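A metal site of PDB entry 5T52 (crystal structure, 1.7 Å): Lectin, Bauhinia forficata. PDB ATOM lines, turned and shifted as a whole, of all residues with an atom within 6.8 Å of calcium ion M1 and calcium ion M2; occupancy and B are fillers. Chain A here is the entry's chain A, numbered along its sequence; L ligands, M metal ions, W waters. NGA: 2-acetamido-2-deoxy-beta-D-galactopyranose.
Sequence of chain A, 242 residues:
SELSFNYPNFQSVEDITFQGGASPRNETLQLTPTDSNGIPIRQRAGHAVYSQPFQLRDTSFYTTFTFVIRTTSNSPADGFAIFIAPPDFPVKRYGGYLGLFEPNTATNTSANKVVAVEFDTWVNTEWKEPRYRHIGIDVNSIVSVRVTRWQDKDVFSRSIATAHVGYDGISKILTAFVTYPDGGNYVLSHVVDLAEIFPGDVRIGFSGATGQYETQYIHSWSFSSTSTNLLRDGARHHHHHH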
ATOM      1  N   ASP A  78       9.804   3.094   5.115  1.00  0.00           N
ATOM      2  CA  ASP A  78       9.951   3.809   3.835  1.00  0.00           C
ATOM      3  C   ASP A  78       9.906   5.268   3.975  1.00  0.00           C
ATOM      4  O   ASP A  78      10.299   5.967   3.059  1.00  0.00           O
ATOM      5  CB  ASP A  78       8.874   3.398   2.804  1.00  0.00           C
ATOM      6  CG  ASP A  78       9.242   2.092   2.172  1.00  0.00           C
ATOM      7  OD1 ASP A  78      10.020   2.139   1.166  1.00  0.00           O
ATOM      8  OD2 ASP A  78       8.848   0.974   2.663  1.00  0.00           O
ATOM      9  N   GLY A  95       4.962   0.129   1.814  1.00  0.00           N
ATOM     10  CA  GLY A  95       6.242   0.099   1.176  1.00  0.00           C
ATOM     11  C   GLY A  95       6.529   1.452   0.547  1.00  0.00           C
ATOM     12  O   GLY A  95       6.114   2.480   1.071  1.00  0.00           O
ATOM     13  N   GLY A  96       7.218   1.447  -0.577  1.00  0.00           N
ATOM     14  CA  GLY A  96       7.677   2.694  -1.184  1.00  0.00           C
ATOM     15  C   GLY A  96       6.612   3.569  -1.756  1.00  0.00           C
ATOM     16  O   GLY A  96       6.884   4.758  -2.056  1.00  0.00           O
ATOM     17  N   TYR A  97       5.371   3.043  -1.802  1.00  0.00           N
ATOM     18  CA  TYR A  97       4.222   3.860  -2.247  1.00  0.00           C
ATOM     19  C   TYR A  97       3.730   4.816  -1.131  1.00  0.00           C
ATOM     20  O   TYR A  97       2.896   5.712  -1.398  1.00  0.00           O
ATOM     21  CB  TYR A  97       3.108   2.955  -2.709  1.00  0.00           C
ATOM     22  CG  TYR A  97       3.543   2.071  -3.819  1.00  0.00           C
ATOM     23  CD1 TYR A  97       3.713   2.580  -5.120  1.00  0.00           C
ATOM     24  CD2 TYR A  97       3.792   0.709  -3.583  1.00  0.00           C
ATOM     25  CE1 TYR A  97       4.177   1.750  -6.175  1.00  0.00           C
ATOM     26  CE2 TYR A  97       4.211  -0.075  -4.590  1.00  0.00           C
ATOM     27  CZ  TYR A  97       4.397   0.427  -5.874  1.00  0.00           C
ATOM     28  OH  TYR A  97       4.806  -0.453  -6.894  1.00  0.00           O
ATOM     29  N   LEU A  98       4.267   4.672   0.104  1.00  0.00           N
ATOM     30  CA  LEU A  98       4.125   5.613   1.178  1.00  0.00           C
ATOM     31  C   LEU A  98       2.682   5.687   1.646  1.00  0.00           C
ATOM     32  O   LEU A  98       2.281   6.678   2.227  1.00  0.00           O
ATOM     33  CB  LEU A  98       4.712   7.025   0.860  1.00  0.00           C
ATOM     34  CG  LEU A  98       6.246   6.957   0.645  1.00  0.00           C
ATOM     35  CD1 LEU A  98       6.726   8.330   0.262  1.00  0.00           C
ATOM     36  CD2 LEU A  98       6.951   6.519   1.915  1.00  0.00           C
ATOM     37  N   GLU A 118       7.110  14.592   0.904  1.00  0.00           N
ATOM     38  CA  GLU A 118       7.475  13.280   1.372  1.00  0.00           C
ATOM     39  C   GLU A 118       8.933  13.301   1.980  1.00  0.00           C
ATOM     40  O   GLU A 118       9.773  14.134   1.583  1.00  0.00           O
ATOM     41  CB  GLU A 118       7.369  12.276   0.213  1.00  0.00           C
ATOM     42  CG  GLU A 118       8.488  12.440  -0.839  1.00  0.00           C
ATOM     43  CD  GLU A 118       8.653  11.290  -1.777  1.00  0.00           C
ATOM     44  OE1 GLU A 118       7.674  10.735  -2.338  1.00  0.00           O
ATOM     45  OE2 GLU A 118       9.827  10.933  -2.034  1.00  0.00           O
ATOM     46  N   ASP A 120      11.657  10.615   2.538  1.00  0.00           N
ATOM     47  CA  ASP A 120      11.806   9.308   1.974  1.00  0.00           C
ATOM     48  C   ASP A 120      13.070   8.690   2.448  1.00  0.00           C
ATOM     49  O   ASP A 120      14.151   9.116   2.067  1.00  0.00           O
ATOM     50  CB  ASP A 120      11.788   9.395   0.388  1.00  0.00           C
ATOM     51  CG  ASP A 120      11.748   8.036  -0.342  1.00  0.00           C
ATOM     52  OD1 ASP A 120      12.125   7.011   0.251  1.00  0.00           O
ATOM     53  OD2 ASP A 120      11.205   7.965  -1.506  1.00  0.00           O
ATOM     54  N   THR A 121      12.945   7.612   3.320  1.00  0.00           N
ATOM     55  CA  THR A 121      14.111   6.942   3.887  1.00  0.00           C
ATOM     56  C   THR A 121      14.706   5.784   3.111  1.00  0.00           C
ATOM     57  O   THR A 121      15.740   5.266   3.488  1.00  0.00           O
ATOM     58  CB  THR A 121      13.777   6.444   5.270  1.00  0.00           C
ATOM     59  OG1 THR A 121      12.726   5.506   5.101  1.00  0.00           O
ATOM     60  CG2 THR A 121      13.428   7.558   6.147  1.00  0.00           C
ATOM     61  N   TRP A 122      14.016   5.379   2.034  1.00  0.00           N
ATOM     62  CA  TRP A 122      14.393   4.159   1.315  1.00  0.00           C
ATOM     63  C   TRP A 122      14.474   4.429  -0.188  1.00  0.00           C
ATOM     64  O   TRP A 122      13.504   4.722  -0.837  1.00  0.00           O
ATOM     65  CB  TRP A 122      13.411   2.995   1.603  1.00  0.00           C
ATOM     66  CG  TRP A 122      13.727   1.771   0.826  1.00  0.00           C
ATOM     67  CD1 TRP A 122      13.318   1.492  -0.465  1.00  0.00           C
ATOM     68  CD2 TRP A 122      14.529   0.687   1.243  1.00  0.00           C
ATOM     69  NE1 TRP A 122      13.844   0.262  -0.863  1.00  0.00           N
ATOM     70  CE2 TRP A 122      14.549  -0.259   0.203  1.00  0.00           C
ATOM     71  CE3 TRP A 122      15.221   0.394   2.440  1.00  0.00           C
ATOM     72  CZ2 TRP A 122      15.321  -1.412   0.288  1.00  0.00           C
ATOM     73  CZ3 TRP A 122      15.916  -0.774   2.514  1.00  0.00           C
ATOM     74  CH2 TRP A 122      15.927  -1.673   1.475  1.00  0.00           C
ATOM     75  N   VAL A 123      15.667   4.260  -0.754  1.00  0.00           N
ATOM     76  CA  VAL A 123      15.823   4.539  -2.143  1.00  0.00           C
ATOM     77  C   VAL A 123      15.193   3.344  -2.910  1.00  0.00           C
ATOM     78  O   VAL A 123      15.752   2.192  -2.821  1.00  0.00           O
ATOM     79  CB  VAL A 123      17.332   4.624  -2.488  1.00  0.00           C
ATOM     80  CG1 VAL A 123      17.501   4.718  -4.012  1.00  0.00           C
ATOM     81  CG2 VAL A 123      17.927   5.868  -1.833  1.00  0.00           C
ATOM     82  N   ASN A 124      14.225   3.601  -3.737  1.00  0.00           N
ATOM     83  CA  ASN A 124      13.557   2.615  -4.569  1.00  0.00           C
ATOM     84  C   ASN A 124      14.129   2.621  -5.968  1.00  0.00           C
ATOM     85  O   ASN A 124      14.409   3.673  -6.521  1.00  0.00           O
ATOM     86  CB  ASN A 124      12.074   2.968  -4.653  1.00  0.00           C
ATOM     87  CG  ASN A 124      11.336   2.641  -3.376  1.00  0.00           C
ATOM     88  OD1 ASN A 124      11.026   3.534  -2.550  1.00  0.00           O
ATOM     89  ND2 ASN A 124      10.952   1.348  -3.237  1.00  0.00           N
ATOM     90  N   TRP A 127      11.158   2.571  -9.459  1.00  0.00           N
ATOM     91  CA  TRP A 127      10.883   3.771 -10.241  1.00  0.00           C
ATOM     92  C   TRP A 127      12.013   4.737 -10.063  1.00  0.00           C
ATOM     93  O   TRP A 127      12.914   4.489  -9.267  1.00  0.00           O
ATOM     94  CB  TRP A 127       9.527   4.403  -9.831  1.00  0.00           C
ATOM     95  CG  TRP A 127       9.426   4.651  -8.321  1.00  0.00           C
ATOM     96  CD1 TRP A 127       9.976   5.677  -7.577  1.00  0.00           C
ATOM     97  CD2 TRP A 127       8.766   3.784  -7.389  1.00  0.00           C
ATOM     98  NE1 TRP A 127       9.714   5.477  -6.246  1.00  0.00           N
ATOM     99  CE2 TRP A 127       8.975   4.311  -6.100  1.00  0.00           C
ATOM    100  CE3 TRP A 127       8.129   2.544  -7.526  1.00  0.00           C
ATOM    101  CZ2 TRP A 127       8.423   3.734  -4.955  1.00  0.00           C
ATOM    102  CZ3 TRP A 127       7.531   1.965  -6.360  1.00  0.00           C
ATOM    103  CH2 TRP A 127       7.779   2.533  -5.083  1.00  0.00           C
ATOM    104  N   LYS A 128      11.952   5.882 -10.760  1.00  0.00           N
ATOM    105  CA  LYS A 128      13.053   6.863 -10.710  1.00  0.00           C
ATOM    106  C   LYS A 128      13.013   7.690  -9.434  1.00  0.00           C
ATOM    107  O   LYS A 128      12.002   8.309  -9.104  1.00  0.00           O
ATOM    108  CB  LYS A 128      13.006   7.802 -11.907  1.00  0.00           C
ATOM    109  CG  LYS A 128      13.381   7.109 -13.227  1.00  0.00           C
ATOM    110  CD  LYS A 128      13.585   8.049 -14.446  1.00  0.00           C
ATOM    111  CE  LYS A 128      14.069   7.311 -15.719  1.00  0.00           C
ATOM    112  NZ  LYS A 128      14.060   8.053 -17.038  1.00  0.00           N
ATOM    113  N   GLU A 129      14.070   7.576  -8.649  1.00  0.00           N
ATOM    114  CA  GLU A 129      14.297   8.541  -7.575  1.00  0.00           C
ATOM    115  C   GLU A 129      15.726   8.608  -7.267  1.00  0.00           C
ATOM    116  O   GLU A 129      16.514   7.838  -7.828  1.00  0.00           O
ATOM    117  CB  GLU A 129      13.409   8.332  -6.353  1.00  0.00           C
ATOM    118  CG  GLU A 129      13.448   6.932  -5.723  1.00  0.00           C
ATOM    119  CD  GLU A 129      12.495   6.770  -4.475  1.00  0.00           C
ATOM    120  OE1 GLU A 129      11.392   7.355  -4.435  1.00  0.00           O
ATOM    121  OE2 GLU A 129      12.862   6.052  -3.539  1.00  0.00           O
ATOM    122  N   PRO A 130      16.120   9.615  -6.482  1.00  0.00           N
ATOM    123  CA  PRO A 130      17.542   9.760  -6.292  1.00  0.00           C
ATOM    124  C   PRO A 130      18.225   8.635  -5.553  1.00  0.00           C
ATOM    125  O   PRO A 130      17.613   7.879  -4.868  1.00  0.00           O
ATOM    126  CB  PRO A 130      17.682  11.057  -5.448  1.00  0.00           C
ATOM    127  CG  PRO A 130      16.329  11.750  -5.480  1.00  0.00           C
ATOM    128  CD  PRO A 130      15.348  10.680  -5.790  1.00  0.00           C
ATOM    129  N   HIS A 134      15.914  11.358   0.630  1.00  0.00           N
ATOM    130  CA  HIS A 134      15.550  12.622   0.040  1.00  0.00           C
ATOM    131  C   HIS A 134      14.229  13.075   0.569  1.00  0.00           C
ATOM    132  O   HIS A 134      13.479  12.268   1.025  1.00  0.00           O
ATOM    133  CB  HIS A 134      15.608  12.503  -1.498  1.00  0.00           C
ATOM    134  CG  HIS A 134      14.762  11.386  -2.061  1.00  0.00           C
ATOM    135  ND1 HIS A 134      15.195  10.086  -2.061  1.00  0.00           N
ATOM    136  CD2 HIS A 134      13.452  11.337  -2.417  1.00  0.00           C
ATOM    137  CE1 HIS A 134      14.244   9.298  -2.536  1.00  0.00           C
ATOM    138  NE2 HIS A 134      13.182  10.020  -2.772  1.00  0.00           N
ATOM    139  N   GLY A 136      10.966  15.427  -0.873  1.00  0.00           N
ATOM    140  CA  GLY A 136      10.372  15.668  -2.174  1.00  0.00           C
ATOM    141  C   GLY A 136       9.031  16.282  -2.129  1.00  0.00           C
ATOM    142  O   GLY A 136       8.313  16.120  -1.167  1.00  0.00           O
ATOM    143  N   ASP A 138       5.585  15.820  -4.254  1.00  0.00           N
ATOM    144  CA  ASP A 138       4.918  14.900  -5.177  1.00  0.00           C
ATOM    145  C   ASP A 138       3.660  15.482  -5.642  1.00  0.00           C
ATOM    146  O   ASP A 138       2.806  15.933  -4.820  1.00  0.00           O
ATOM    147  CB  ASP A 138       4.567  13.620  -4.407  1.00  0.00           C
ATOM    148  CG  ASP A 138       5.807  12.891  -3.838  1.00  0.00           C
ATOM    149  OD1 ASP A 138       6.943  13.113  -4.325  1.00  0.00           O
ATOM    150  OD2 ASP A 138       5.628  11.992  -2.922  1.00  0.00           O
ATOM    151  N   ILE A 142       4.258   9.099  -7.512  1.00  0.00           N
ATOM    152  CA  ILE A 142       5.330   8.724  -6.553  1.00  0.00           C
ATOM    153  C   ILE A 142       6.749   9.151  -6.988  1.00  0.00           C
ATOM    154  O   ILE A 142       7.685   9.276  -6.146  1.00  0.00           O
ATOM    155  CB  ILE A 142       5.328   7.187  -6.286  1.00  0.00           C
ATOM    156  CG1 ILE A 142       6.056   6.836  -4.945  1.00  0.00           C
ATOM    157  CG2 ILE A 142       5.883   6.417  -7.480  1.00  0.00           C
ATOM    158  CD1 ILE A 142       5.619   7.496  -3.642  1.00  0.00           C
ATOM    159  N   VAL A 143       6.864   9.548  -8.241  1.00  0.00           N
ATOM    160  CA  VAL A 143       8.113  10.137  -8.755  1.00  0.00           C
ATOM    161  C   VAL A 143       8.034  11.667  -8.534  1.00  0.00           C
ATOM    162  O   VAL A 143       7.253  12.398  -9.165  1.00  0.00           O
ATOM    163  CB  VAL A 143       8.353   9.816 -10.262  1.00  0.00           C
ATOM    164  CG1 VAL A 143       9.610  10.453 -10.737  1.00  0.00           C
ATOM    165  CG2 VAL A 143       8.511   8.312 -10.397  1.00  0.00           C
ATOM    166  N   SER A 144       8.791  12.145  -7.555  1.00  0.00           N
ATOM    167  CA  SER A 144       8.680  13.547  -7.171  1.00  0.00           C
ATOM    168  C   SER A 144       9.015  14.485  -8.271  1.00  0.00           C
ATOM    169  O   SER A 144       9.974  14.287  -9.016  1.00  0.00           O
ATOM    170  CB  SER A 144       9.629  13.870  -5.990  1.00  0.00           C
ATOM    171  OG  SER A 144       9.470  12.946  -4.886  1.00  0.00           O
ATOM    172  N   VAL A 147      12.996  17.397  -5.764  1.00  0.00           N
ATOM    173  CA  VAL A 147      13.591  16.545  -4.760  1.00  0.00           C
ATOM    174  C   VAL A 147      14.917  17.133  -4.305  1.00  0.00           C
ATOM    175  O   VAL A 147      15.578  17.816  -5.063  1.00  0.00           O
ATOM    176  CB  VAL A 147      13.666  15.106  -5.382  1.00  0.00           C
ATOM    177  CG1 VAL A 147      14.849  14.906  -6.386  1.00  0.00           C
ATOM    178  CG2 VAL A 147      13.657  14.163  -4.283  1.00  0.00           C
HETATM  179  C1  NGA L   1      10.602  -3.345  -1.063  1.00  0.00           C
HETATM  180  C2  NGA L   1       9.775  -2.057  -1.155  1.00  0.00           C
HETATM  181  C3  NGA L   1      10.549  -0.868  -0.648  1.00  0.00           C
HETATM  182  C4  NGA L   1      10.969  -1.134   0.812  1.00  0.00           C
HETATM  183  C5  NGA L   1      11.640  -2.507   0.809  1.00  0.00           C
HETATM  184  C6  NGA L   1      12.013  -2.902   2.220  1.00  0.00           C
HETATM  185  C7  NGA L   1       8.206  -1.337  -2.904  1.00  0.00           C
HETATM  186  C8  NGA L   1       7.900  -1.142  -4.341  1.00  0.00           C
HETATM  187  N2  NGA L   1       9.366  -1.793  -2.565  1.00  0.00           N
HETATM  188  O1  NGA L   1       9.856  -4.456  -1.455  1.00  0.00           O
HETATM  189  O3  NGA L   1       9.867   0.360  -0.833  1.00  0.00           O
HETATM  190  O4  NGA L   1       9.819  -1.205   1.630  1.00  0.00           O
HETATM  191  O5  NGA L   1      10.891  -3.603   0.324  1.00  0.00           O
HETATM  192  O6  NGA L   1      12.672  -4.184   2.310  1.00  0.00           O
HETATM  193  O7  NGA L   1       7.328  -1.065  -2.099  1.00  0.00           O
HETATM  194 CA    CA M   1      11.428   5.591  -1.601  1.00  0.00          CA
HETATM  195 CA    CA M   2      10.862   9.310  -3.256  1.00  0.00          CA
HETATM  196  O   HOH W   1       8.585   8.644  -3.590  1.00  0.00           O
HETATM  197  O   HOH W   2      10.919  10.690  -4.988  1.00  0.00           O
HETATM  198  O   HOH W   3       9.227   6.033  -2.452  1.00  0.00           O
HETATM  199  O   HOH W   4      10.345   4.704   0.383  1.00  0.00           O
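Water W1 lies within hydrogen-bond range of OE1 of Glu 118 and O of Ile 142.
The nearest printed residue that does not touch calcium ion M2 is Ser 144 (4.2 Å).
OE1 of Glu 118 lies close to OD2 of Asp 138 (2.5 Å). The backbone carbonyl oxygen (O) of Gly 136 is in hydrogen-bond range of the backbone NH (N) of Glu 118 (2.8 Å). The side-chain carboxylate (OE1) of Glu 129 lies close to the indole nitrogen (NE1) of Trp 127 (3.1 Å).
ND2 of Asn 124 is in hydrogen-bond range of O3 of the ligand. O3 of the ligand is in hydrogen-bond range of N of Gly 96 (2.9 Å). An oxygen (O4) of the ligand sits at hydrogen-bond distance from the side-chain carboxylate (OD2) of Asp 78 (2.6 Å).
Four residues have an atom within 4 Å of calcium ion M1: Asp 120, Trp 122, Asn 124 and Glu 129. Along chain A the residues within 4 Å of calcium ion M1 span positions 120 to 129. The nearest printed residue that does not touch calcium ion M1 is Val 123 (4.5 Å).
Calcium ion M2 is bound by water W2 (2.2 Å). OD2 of Asp 120 is bound to calcium ion M2, 2.2 Å away. Calcium ion M2 is bound by OE2 of Glu 118 (2.3 Å). OE1 of Glu 129 is bound to calcium ion M2, at 2.3 Å. Calcium ion M2 is bound by water W1 (2.4 Å). NE2 of His 134 is bound to calcium ion M2 (2.5 Å).
Calcium ion M1 is bound by OD1 of Asn 124 (2.3 Å), O of Trp 122 (2.4 Å), OD2 of Asp 120 (2.4 Å), water W3 (2.4 Å), water W4 (2.4 Å), OD1 of Asp 120 (2.4 Å) and OE2 of Glu 129 (2.5 Å).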
